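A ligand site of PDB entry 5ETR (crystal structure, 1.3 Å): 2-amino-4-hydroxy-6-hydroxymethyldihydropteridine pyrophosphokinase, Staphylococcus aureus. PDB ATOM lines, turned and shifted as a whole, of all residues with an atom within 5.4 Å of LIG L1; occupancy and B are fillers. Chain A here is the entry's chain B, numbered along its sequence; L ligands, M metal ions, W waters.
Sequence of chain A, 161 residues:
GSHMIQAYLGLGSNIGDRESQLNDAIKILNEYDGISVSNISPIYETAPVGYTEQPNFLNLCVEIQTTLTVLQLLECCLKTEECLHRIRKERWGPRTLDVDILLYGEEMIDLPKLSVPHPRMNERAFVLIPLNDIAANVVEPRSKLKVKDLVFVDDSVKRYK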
ATOM      1  N   GLY A  12      -0.645  -7.882   0.987  1.00  0.00           N
ATOM      2  CA  GLY A  12      -1.759  -8.314   1.776  1.00  0.00           C
ATOM      3  C   GLY A  12      -1.945  -7.460   3.014  1.00  0.00           C
ATOM      4  O   GLY A  12      -0.986  -6.957   3.560  1.00  0.00           O
ATOM      5  N   ASN A  14      -4.761  -7.674   6.607  1.00  0.00           N
ATOM      6  CA  ASN A  14      -5.949  -8.241   7.234  1.00  0.00           C
ATOM      7  C   ASN A  14      -6.315  -7.631   8.589  1.00  0.00           C
ATOM      8  O   ASN A  14      -7.053  -8.231   9.367  1.00  0.00           O
ATOM      9  CB  ASN A  14      -5.947  -9.779   7.237  1.00  0.00           C
ATOM     10  CG  ASN A  14      -4.967 -10.369   8.230  1.00  0.00           C
ATOM     11  OD1 ASN A  14      -3.920  -9.800   8.512  1.00  0.00           O
ATOM     12  ND2 ASN A  14      -5.306 -11.537   8.765  1.00  0.00           N
ATOM     13  N   THR A  46      -9.985 -12.119   0.323  1.00  0.00           N
ATOM     14  CA  THR A  46      -9.599 -13.506   0.261  1.00  0.00           C
ATOM     15  C   THR A  46      -9.663 -14.114   1.641  1.00  0.00           C
ATOM     16  O   THR A  46      -9.281 -13.544   2.656  1.00  0.00           O
ATOM     17  CB  THR A  46      -8.182 -13.671  -0.350  1.00  0.00           C
ATOM     18  OG1 THR A  46      -7.210 -13.156   0.562  1.00  0.00           O
ATOM     19  CG2 THR A  46      -8.071 -12.909  -1.694  1.00  0.00           C
ATOM     20  N   ALA A  47     -10.066 -15.402   1.660  1.00  0.00           N
ATOM     21  CA  ALA A  47     -10.074 -16.199   2.912  1.00  0.00           C
ATOM     22  C   ALA A  47      -8.636 -16.534   3.304  1.00  0.00           C
ATOM     23  O   ALA A  47      -7.863 -16.953   2.443  1.00  0.00           O
ATOM     24  CB  ALA A  47     -10.886 -17.455   2.729  1.00  0.00           C
ATOM     25  N   PRO A  48      -8.310 -16.411   4.594  1.00  0.00           N
ATOM     26  CA  PRO A  48      -6.996 -16.801   5.030  1.00  0.00           C
ATOM     27  C   PRO A  48      -6.721 -18.283   4.771  1.00  0.00           C
ATOM     28  O   PRO A  48      -7.594 -19.154   4.992  1.00  0.00           O
ATOM     29  CB  PRO A  48      -6.997 -16.554   6.520  1.00  0.00           C
ATOM     30  CG  PRO A  48      -8.049 -15.537   6.718  1.00  0.00           C
ATOM     31  CD  PRO A  48      -9.103 -15.863   5.709  1.00  0.00           C
ATOM     32  N   VAL A  49      -5.475 -18.558   4.327  1.00  0.00           N
ATOM     33  CA  VAL A  49      -5.015 -19.929   4.223  1.00  0.00           C
ATOM     34  C   VAL A  49      -3.788 -20.151   5.081  1.00  0.00           C
ATOM     35  O   VAL A  49      -3.022 -19.247   5.382  1.00  0.00           O
ATOM     36  CB  VAL A  49      -4.742 -20.348   2.763  1.00  0.00           C
ATOM     37  CG1 VAL A  49      -6.007 -20.230   1.920  1.00  0.00           C
ATOM     38  CG2 VAL A  49      -3.621 -19.517   2.158  1.00  0.00           C
ATOM     39  N   GLY A  50      -3.607 -21.441   5.460  1.00  0.00           N
ATOM     40  CA  GLY A  50      -2.404 -21.871   6.099  1.00  0.00           C
ATOM     41  C   GLY A  50      -2.303 -21.638   7.585  1.00  0.00           C
ATOM     42  O   GLY A  50      -1.259 -21.809   8.200  1.00  0.00           O
ATOM     43  N   TYR A  51      -3.411 -21.285   8.207  1.00  0.00           N
ATOM     44  CA  TYR A  51      -3.370 -20.991   9.657  1.00  0.00           C
ATOM     45  C   TYR A  51      -4.755 -21.309  10.266  1.00  0.00           C
ATOM     46  O   TYR A  51      -5.495 -22.114   9.742  1.00  0.00           O
ATOM     47  CB  TYR A  51      -2.882 -19.569   9.851  1.00  0.00           C
ATOM     48  CG  TYR A  51      -2.300 -19.194  11.199  1.00  0.00           C
ATOM     49  CD1 TYR A  51      -1.374 -19.957  11.828  1.00  0.00           C
ATOM     50  CD2 TYR A  51      -2.612 -17.973  11.772  1.00  0.00           C
ATOM     51  CE1 TYR A  51      -0.809 -19.573  13.045  1.00  0.00           C
ATOM     52  CE2 TYR A  51      -2.109 -17.585  12.982  1.00  0.00           C
ATOM     53  CZ  TYR A  51      -1.189 -18.384  13.635  1.00  0.00           C
ATOM     54  OH  TYR A  51      -0.600 -18.035  14.818  1.00  0.00           O
ATOM     55  N   THR A  52      -5.043 -20.757  11.404  1.00  0.00           N
ATOM     56  CA  THR A  52      -6.366 -20.844  12.021  1.00  0.00           C
ATOM     57  C   THR A  52      -7.293 -19.814  11.390  1.00  0.00           C
ATOM     58  O   THR A  52      -6.901 -19.035  10.515  1.00  0.00           O
ATOM     59  CB  THR A  52      -6.188 -20.581  13.541  1.00  0.00           C
ATOM     60  OG1 THR A  52      -5.447 -19.353  13.722  1.00  0.00           O
ATOM     61  CG2 THR A  52      -5.467 -21.693  14.164  1.00  0.00           C
ATOM     62  N   GLN A  54      -9.011 -16.490  10.787  1.00  0.00           N
ATOM     63  CA  GLN A  54      -8.410 -15.156  10.938  1.00  0.00           C
ATOM     64  C   GLN A  54      -9.268 -14.205  10.139  1.00  0.00           C
ATOM     65  O   GLN A  54     -10.066 -14.638   9.283  1.00  0.00           O
ATOM     66  CB  GLN A  54      -6.986 -15.124  10.413  1.00  0.00           C
ATOM     67  CG  GLN A  54      -6.020 -15.943  11.240  1.00  0.00           C
ATOM     68  CD  GLN A  54      -5.803 -15.401  12.649  1.00  0.00           C
ATOM     69  OE1 GLN A  54      -5.995 -14.200  12.910  1.00  0.00           O
ATOM     70  NE2 GLN A  54      -5.422 -16.285  13.561  1.00  0.00           N
ATOM     71  N   PRO A  55      -9.141 -12.908  10.368  1.00  0.00           N
ATOM     72  CA  PRO A  55      -9.912 -11.967   9.548  1.00  0.00           C
ATOM     73  C   PRO A  55      -9.508 -12.072   8.082  1.00  0.00           C
ATOM     74  O   PRO A  55      -8.386 -12.342   7.779  1.00  0.00           O
ATOM     75  CB  PRO A  55      -9.553 -10.600  10.112  1.00  0.00           C
ATOM     76  CG  PRO A  55      -8.535 -10.819  11.140  1.00  0.00           C
ATOM     77  CD  PRO A  55      -8.426 -12.269  11.466  1.00  0.00           C
ATOM     78  N   PHE A  57      -8.414 -11.220   4.307  1.00  0.00           N
ATOM     79  CA  PHE A  57      -7.394 -10.345   3.712  1.00  0.00           C
ATOM     80  C   PHE A  57      -7.984  -9.526   2.577  1.00  0.00           C
ATOM     81  O   PHE A  57      -8.876  -9.945   1.911  1.00  0.00           O
ATOM     82  CB  PHE A  57      -6.298 -11.217   3.078  1.00  0.00           C
ATOM     83  CG  PHE A  57      -5.309 -11.785   4.064  1.00  0.00           C
ATOM     84  CD1 PHE A  57      -5.547 -12.998   4.641  1.00  0.00           C
ATOM     85  CD2 PHE A  57      -4.163 -11.106   4.382  1.00  0.00           C
ATOM     86  CE1 PHE A  57      -4.658 -13.532   5.539  1.00  0.00           C
ATOM     87  CE2 PHE A  57      -3.271 -11.623   5.294  1.00  0.00           C
ATOM     88  CZ  PHE A  57      -3.522 -12.853   5.859  1.00  0.00           C
ATOM     89  N   ASN A  59      -5.943  -8.658  -0.761  1.00  0.00           N
ATOM     90  CA  ASN A  59      -4.721  -8.986  -1.474  1.00  0.00           C
ATOM     91  C   ASN A  59      -4.710  -8.405  -2.860  1.00  0.00           C
ATOM     92  O   ASN A  59      -5.751  -8.278  -3.507  1.00  0.00           O
ATOM     93  CB  ASN A  59      -4.570 -10.534  -1.639  1.00  0.00           C
ATOM     94  CG  ASN A  59      -4.108 -11.261  -0.383  1.00  0.00           C
ATOM     95  OD1 ASN A  59      -4.799 -12.132   0.177  1.00  0.00           O
ATOM     96  ND2 ASN A  59      -2.881 -10.985   0.025  1.00  0.00           N
ATOM     97  N   TRP A  92       2.158 -15.986  14.732  1.00  0.00           N
ATOM     98  CA  TRP A  92       1.623 -15.236  13.621  1.00  0.00           C
ATOM     99  C   TRP A  92       0.215 -14.729  13.974  1.00  0.00           C
ATOM    100  O   TRP A  92      -0.566 -15.324  14.741  1.00  0.00           O
ATOM    101  CB  TRP A  92       1.478 -16.070  12.362  1.00  0.00           C
ATOM    102  CG  TRP A  92       2.710 -16.781  11.895  1.00  0.00           C
ATOM    103  CD1 TRP A  92       4.006 -16.503  12.142  1.00  0.00           C
ATOM    104  CD2 TRP A  92       2.713 -17.981  11.107  1.00  0.00           C
ATOM    105  NE1 TRP A  92       4.825 -17.434  11.552  1.00  0.00           N
ATOM    106  CE2 TRP A  92       4.034 -18.338  10.880  1.00  0.00           C
ATOM    107  CE3 TRP A  92       1.673 -18.779  10.562  1.00  0.00           C
ATOM    108  CZ2 TRP A  92       4.349 -19.476  10.168  1.00  0.00           C
ATOM    109  CZ3 TRP A  92       1.971 -19.880   9.872  1.00  0.00           C
ATOM    110  CH2 TRP A  92       3.316 -20.210   9.657  1.00  0.00           C
ATOM    111  N   GLY A  93      -0.122 -13.600  13.381  1.00  0.00           N
ATOM    112  CA  GLY A  93      -1.491 -13.079  13.477  1.00  0.00           C
ATOM    113  C   GLY A  93      -1.792 -12.103  12.361  1.00  0.00           C
ATOM    114  O   GLY A  93      -1.008 -11.959  11.406  1.00  0.00           O
ATOM    115  N   PRO A  94      -2.925 -11.430  12.464  1.00  0.00           N
ATOM    116  CA  PRO A  94      -3.280 -10.429  11.480  1.00  0.00           C
ATOM    117  C   PRO A  94      -2.155  -9.373  11.344  1.00  0.00           C
ATOM    118  O   PRO A  94      -1.437  -9.084  12.309  1.00  0.00           O
ATOM    119  CB  PRO A  94      -4.556  -9.818  12.080  1.00  0.00           C
ATOM    120  CG  PRO A  94      -5.094 -10.926  12.941  1.00  0.00           C
ATOM    121  CD  PRO A  94      -3.905 -11.555  13.557  1.00  0.00           C
ATOM    122  N   ARG A  95      -2.026  -8.817  10.137  1.00  0.00           N
ATOM    123  CA  ARG A  95      -0.948  -7.863   9.872  1.00  0.00           C
ATOM    124  C   ARG A  95      -1.496  -6.715   9.045  1.00  0.00           C
ATOM    125  O   ARG A  95      -2.294  -6.869   8.137  1.00  0.00           O
ATOM    126  CB  ARG A  95       0.257  -8.481   9.222  1.00  0.00           C
ATOM    127  CG  ARG A  95       0.118  -9.053   7.844  1.00  0.00           C
ATOM    128  CD  ARG A  95      -0.692 -10.364   7.721  1.00  0.00           C
ATOM    129  NE  ARG A  95      -0.104 -11.371   8.594  1.00  0.00           N
ATOM    130  CZ  ARG A  95       0.923 -12.166   8.274  1.00  0.00           C
ATOM    131  NH1 ARG A  95       1.349 -12.298   7.016  1.00  0.00           N
ATOM    132  NH2 ARG A  95       1.534 -12.850   9.259  1.00  0.00           N
ATOM    133  N   ASP A  98       1.725  -6.951   4.386  1.00  0.00           N
ATOM    134  CA  ASP A  98       2.705  -7.971   3.983  1.00  0.00           C
ATOM    135  C   ASP A  98       3.084  -7.683   2.548  1.00  0.00           C
ATOM    136  O   ASP A  98       2.199  -7.574   1.719  1.00  0.00           O
ATOM    137  CB  ASP A  98       2.056  -9.372   4.099  1.00  0.00           C
ATOM    138  CG  ASP A  98       3.009 -10.531   3.816  1.00  0.00           C
ATOM    139  OD1 ASP A  98       4.169 -10.451   4.245  1.00  0.00           O
ATOM    140  OD2 ASP A  98       2.568 -11.523   3.104  1.00  0.00           O
ATOM    141  N   ARG A 124      -1.413 -20.847  -4.405  1.00  0.00           N
ATOM    142  CA  ARG A 124      -2.181 -19.797  -3.714  1.00  0.00           C
ATOM    143  C   ARG A 124      -3.051 -19.026  -4.667  1.00  0.00           C
ATOM    144  O   ARG A 124      -2.537 -18.222  -5.446  1.00  0.00           O
ATOM    145  CB  ARG A 124      -1.267 -18.818  -2.987  1.00  0.00           C
ATOM    146  CG  ARG A 124      -0.709 -19.420  -1.712  1.00  0.00           C
ATOM    147  CD  ARG A 124       0.395 -18.608  -1.104  1.00  0.00           C
ATOM    148  NE  ARG A 124       0.591 -18.916   0.302  1.00  0.00           N
ATOM    149  CZ  ARG A 124       1.333 -18.210   1.138  1.00  0.00           C
ATOM    150  NH1 ARG A 124       2.039 -17.161   0.699  1.00  0.00           N
ATOM    151  NH2 ARG A 124       1.332 -18.533   2.424  1.00  0.00           N
ATOM    152  N   PHE A 126      -4.951 -16.566  -3.819  1.00  0.00           N
ATOM    153  CA  PHE A 126      -4.880 -15.150  -3.468  1.00  0.00           C
ATOM    154  C   PHE A 126      -3.674 -14.479  -4.106  1.00  0.00           C
ATOM    155  O   PHE A 126      -3.645 -13.219  -4.159  1.00  0.00           O
ATOM    156  CB  PHE A 126      -4.888 -14.937  -1.964  1.00  0.00           C
ATOM    157  CG  PHE A 126      -3.588 -15.255  -1.247  1.00  0.00           C
ATOM    158  CD1 PHE A 126      -2.592 -14.322  -1.216  1.00  0.00           C
ATOM    159  CD2 PHE A 126      -3.429 -16.455  -0.528  1.00  0.00           C
ATOM    160  CE1 PHE A 126      -1.399 -14.577  -0.526  1.00  0.00           C
ATOM    161  CE2 PHE A 126      -2.282 -16.693   0.186  1.00  0.00           C
ATOM    162  CZ  PHE A 126      -1.262 -15.765   0.189  1.00  0.00           C
HETATM  163  C1  LIG L   1      -0.758 -15.726   8.725  1.00  0.00           C
HETATM  164  C2  LIG L   1      -2.744 -16.582   7.797  1.00  0.00           C
HETATM  165  C3  LIG L   1      -1.442 -14.743   9.425  1.00  0.00           C
HETATM  166  C4  LIG L   1      -3.446 -15.590   8.460  1.00  0.00           C
HETATM  167  C5  LIG L   1      -1.362 -16.649   7.916  1.00  0.00           C
HETATM  168  C6  LIG L   1      -2.803 -14.718   9.260  1.00  0.00           C
HETATM  169  C7  LIG L   1      -1.863 -14.914   3.384  1.00  0.00           C
HETATM  170  C8  LIG L   1      -2.693 -15.973   3.615  1.00  0.00           C
HETATM  171  C9  LIG L   1      -0.740 -16.250   4.574  1.00  0.00           C
HETATM  172  C10 LIG L   1      -2.342 -13.847   2.544  1.00  0.00           C
HETATM  173  C11 LIG L   1      -4.402 -15.149   2.449  1.00  0.00           C
HETATM  174  C12 LIG L   1      -0.535 -17.677   7.114  1.00  0.00           C
HETATM  175  N1  LIG L   1      -0.645 -15.072   3.998  1.00  0.00           N
HETATM  176  N2  LIG L   1      -3.946 -16.130   3.230  1.00  0.00           N
HETATM  177  N3  LIG L   1      -1.979 -16.814   4.406  1.00  0.00           N
HETATM  178  N4  LIG L   1      -3.640 -14.049   2.137  1.00  0.00           N
HETATM  179  N5  LIG L   1      -5.623 -15.164   1.922  1.00  0.00           N
HETATM  180  O1  LIG L   1      -1.723 -12.812   2.183  1.00  0.00           O
HETATM  181  F1  LIG L   1      -3.496 -13.755   9.916  1.00  0.00           F
HETATM  182  S1  LIG L   1       0.519 -16.989   5.538  1.00  0.00           S
HETATM  183  P1  LG2 L   2       4.374 -16.347   3.430  1.00  0.00           P
HETATM  184  O1  LG2 L   2       3.503 -15.453   2.568  1.00  0.00           O
HETATM  185  O2  LG2 L   2       5.766 -16.386   2.999  1.00  0.00           O
HETATM  186  O3  LG2 L   2       3.839 -17.735   3.651  1.00  0.00           O
HETATM  187  P2  LG2 L   2       4.751 -14.219   5.377  1.00  0.00           P
HETATM  188  O4  LG2 L   2       4.731 -13.342   4.138  1.00  0.00           O
HETATM  189  O5  LG2 L   2       3.798 -13.830   6.457  1.00  0.00           O
HETATM  190  O6  LG2 L   2       4.420 -15.699   4.950  1.00  0.00           O
HETATM  191  P3  LG2 L   2       6.965 -12.737   6.674  1.00  0.00           P
HETATM  192  O7  LG2 L   2       6.353 -11.634   5.880  1.00  0.00           O
HETATM  193  O8  LG2 L   2       6.785 -12.691   8.134  1.00  0.00           O
HETATM  194  C1  LG2 L   2       6.427 -14.335   6.032  1.00  0.00           C
HETATM  195  O9  LG2 L   2       8.504 -12.623   6.311  1.00  0.00           O
HETATM  196  C2  LG2 L   2       9.461 -13.410   7.044  1.00  0.00           C
HETATM  197  C3  LG2 L   2      10.747 -13.415   6.246  1.00  0.00           C
HETATM  198  O10 LG2 L   2      10.548 -14.070   4.975  1.00  0.00           O
HETATM  199  C4  LG2 L   2      11.345 -12.059   5.784  1.00  0.00           C
HETATM  200  O11 LG2 L   2      12.050 -11.388   6.787  1.00  0.00           O
HETATM  201  C5  LG2 L   2      12.268 -12.446   4.607  1.00  0.00           C
HETATM  202  O12 LG2 L   2      13.658 -12.484   5.014  1.00  0.00           O
HETATM  203  C6  LG2 L   2      11.762 -13.836   4.225  1.00  0.00           C
HETATM  204  N1  LG2 L   2      11.465 -14.058   2.823  1.00  0.00           N
HETATM  205  C7  LG2 L   2      11.871 -15.169   2.109  1.00  0.00           C
HETATM  206  N2  LG2 L   2      11.480 -15.172   0.850  1.00  0.00           N
HETATM  207  C8  LG2 L   2      10.755 -13.992   0.756  1.00  0.00           C
HETATM  208  C9  LG2 L   2      10.067 -13.420  -0.311  1.00  0.00           C
HETATM  209  N3  LG2 L   2       9.975 -14.023  -1.560  1.00  0.00           N
HETATM  210  N4  LG2 L   2       9.480 -12.204  -0.132  1.00  0.00           N
HETATM  211  C10 LG2 L   2       9.523 -11.631   1.078  1.00  0.00           C
HETATM  212  N5  LG2 L   2      10.163 -12.102   2.157  1.00  0.00           N
HETATM  213  C11 LG2 L   2      10.761 -13.278   1.933  1.00  0.00           C
HETATM  214 MG    MG M   1       3.067 -13.495   2.792  1.00  0.00          MG
HETATM  215  O   HOH W   1       1.793 -13.954   4.392  1.00  0.00           O
HETATM  216  O   HOH W   2       1.282 -13.637   1.650  1.00  0.00           O
HETATM  217  O   HOH W   3      -0.117 -11.585   4.394  1.00  0.00           O
HETATM  218  O   HOH W   4       2.936 -17.644   7.665  1.00  0.00           O
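A nitrogen (N2) of LIG L1 is in hydrogen-bond range of the backbone NH (N) of Val 49 (3.1 Å).
N3 of LIG L1 sits close to O of Val 49 (2.8 Å).
A nitrogen (N5) of LIG L1 lies within hydrogen-bond range of the side-chain hydroxyl (OG1) of Thr 46.
A nitrogen (N5) of LIG L1 sits at hydrogen-bond distance from the backbone carbonyl oxygen (O) of Ala 47 (2.9 Å).
The side-chain amide oxygen (OD1) of Asn 59 lies within hydrogen-bond range of a nitrogen (N4) of LIG L1 (3.0 Å).
NH2 of Arg 124 lies close to S1 of LIG L1 (3.6 Å).
The guanidinium group (NH1) of Arg 95 lies within salt-bridge range of an oxygen (O5) of LG2 L2.
NH2 of Arg 124 is in salt-bridge range of O3 of LG2 L2 (2.9 Å).
Water W1 lies within hydrogen-bond range of a nitrogen (N1) of LIG L1, an oxygen (O5) of LG2 L2 and the guanidinium group of Arg 95.
Water W3 lies within hydrogen-bond range of an oxygen (O1) of LIG L1 and the guanidinium group of Arg 95.
The side-chain amide nitrogen (ND2) of Asn 14 sits close to a fluorine (F1) of LIG L1, at 3.1 Å.
F1 of LIG L1 sits close to O of Gly 93, 3.4 Å away.
The backbone nitrogen (N) of Pro 94 sits close to a fluorine (F1) of LIG L1 (3.5 Å).
Merely in contact with LIG L1: Pro 48 (3.6 Å), Tyr 51 (3.6 Å), Gln 54 (3.6 Å), Phe 57 (3.3 Å), Arg 95 (3.5 Å) and Phe 126 (3.2 Å).
Hydrophobic or aromatic side chains that line LIG L1: Val 49, Tyr 51, Phe 57 and Phe 126.
Of the 20 residues printed, 14 come within 4 Å of LIG L1.
The nearest printed residue that does not touch LIG L1 is Trp 92 (4.2 Å).
The side-chain amide oxygen (OD1) of Asn 59 is in hydrogen-bond range of the side-chain hydroxyl (OG1) of Thr 46 (2.6 Å).
The backbone NH (N) of Thr 46 lies within hydrogen-bond range of the backbone carbonyl oxygen (O) of Phe 57, at 2.9 Å.
The side-chain amide oxygen (OD1) of Asn 14 is in hydrogen-bond range of the backbone NH (N) of Arg 95 (2.7 Å).
O of Pro 55 lies within hydrogen-bond range of ND2 of Asn 14 (3.3 Å).
O of Gly 93 sits at hydrogen-bond distance from NE of Arg 95, 3.0 Å away.
The side-chain amide nitrogen of Gln 54 sits at hydrogen-bond distance from the side-chain hydroxyl of Thr 52 (3.1 Å).
OH of Tyr 51 lies within hydrogen-bond range of O of Trp 92 (2.7 Å).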
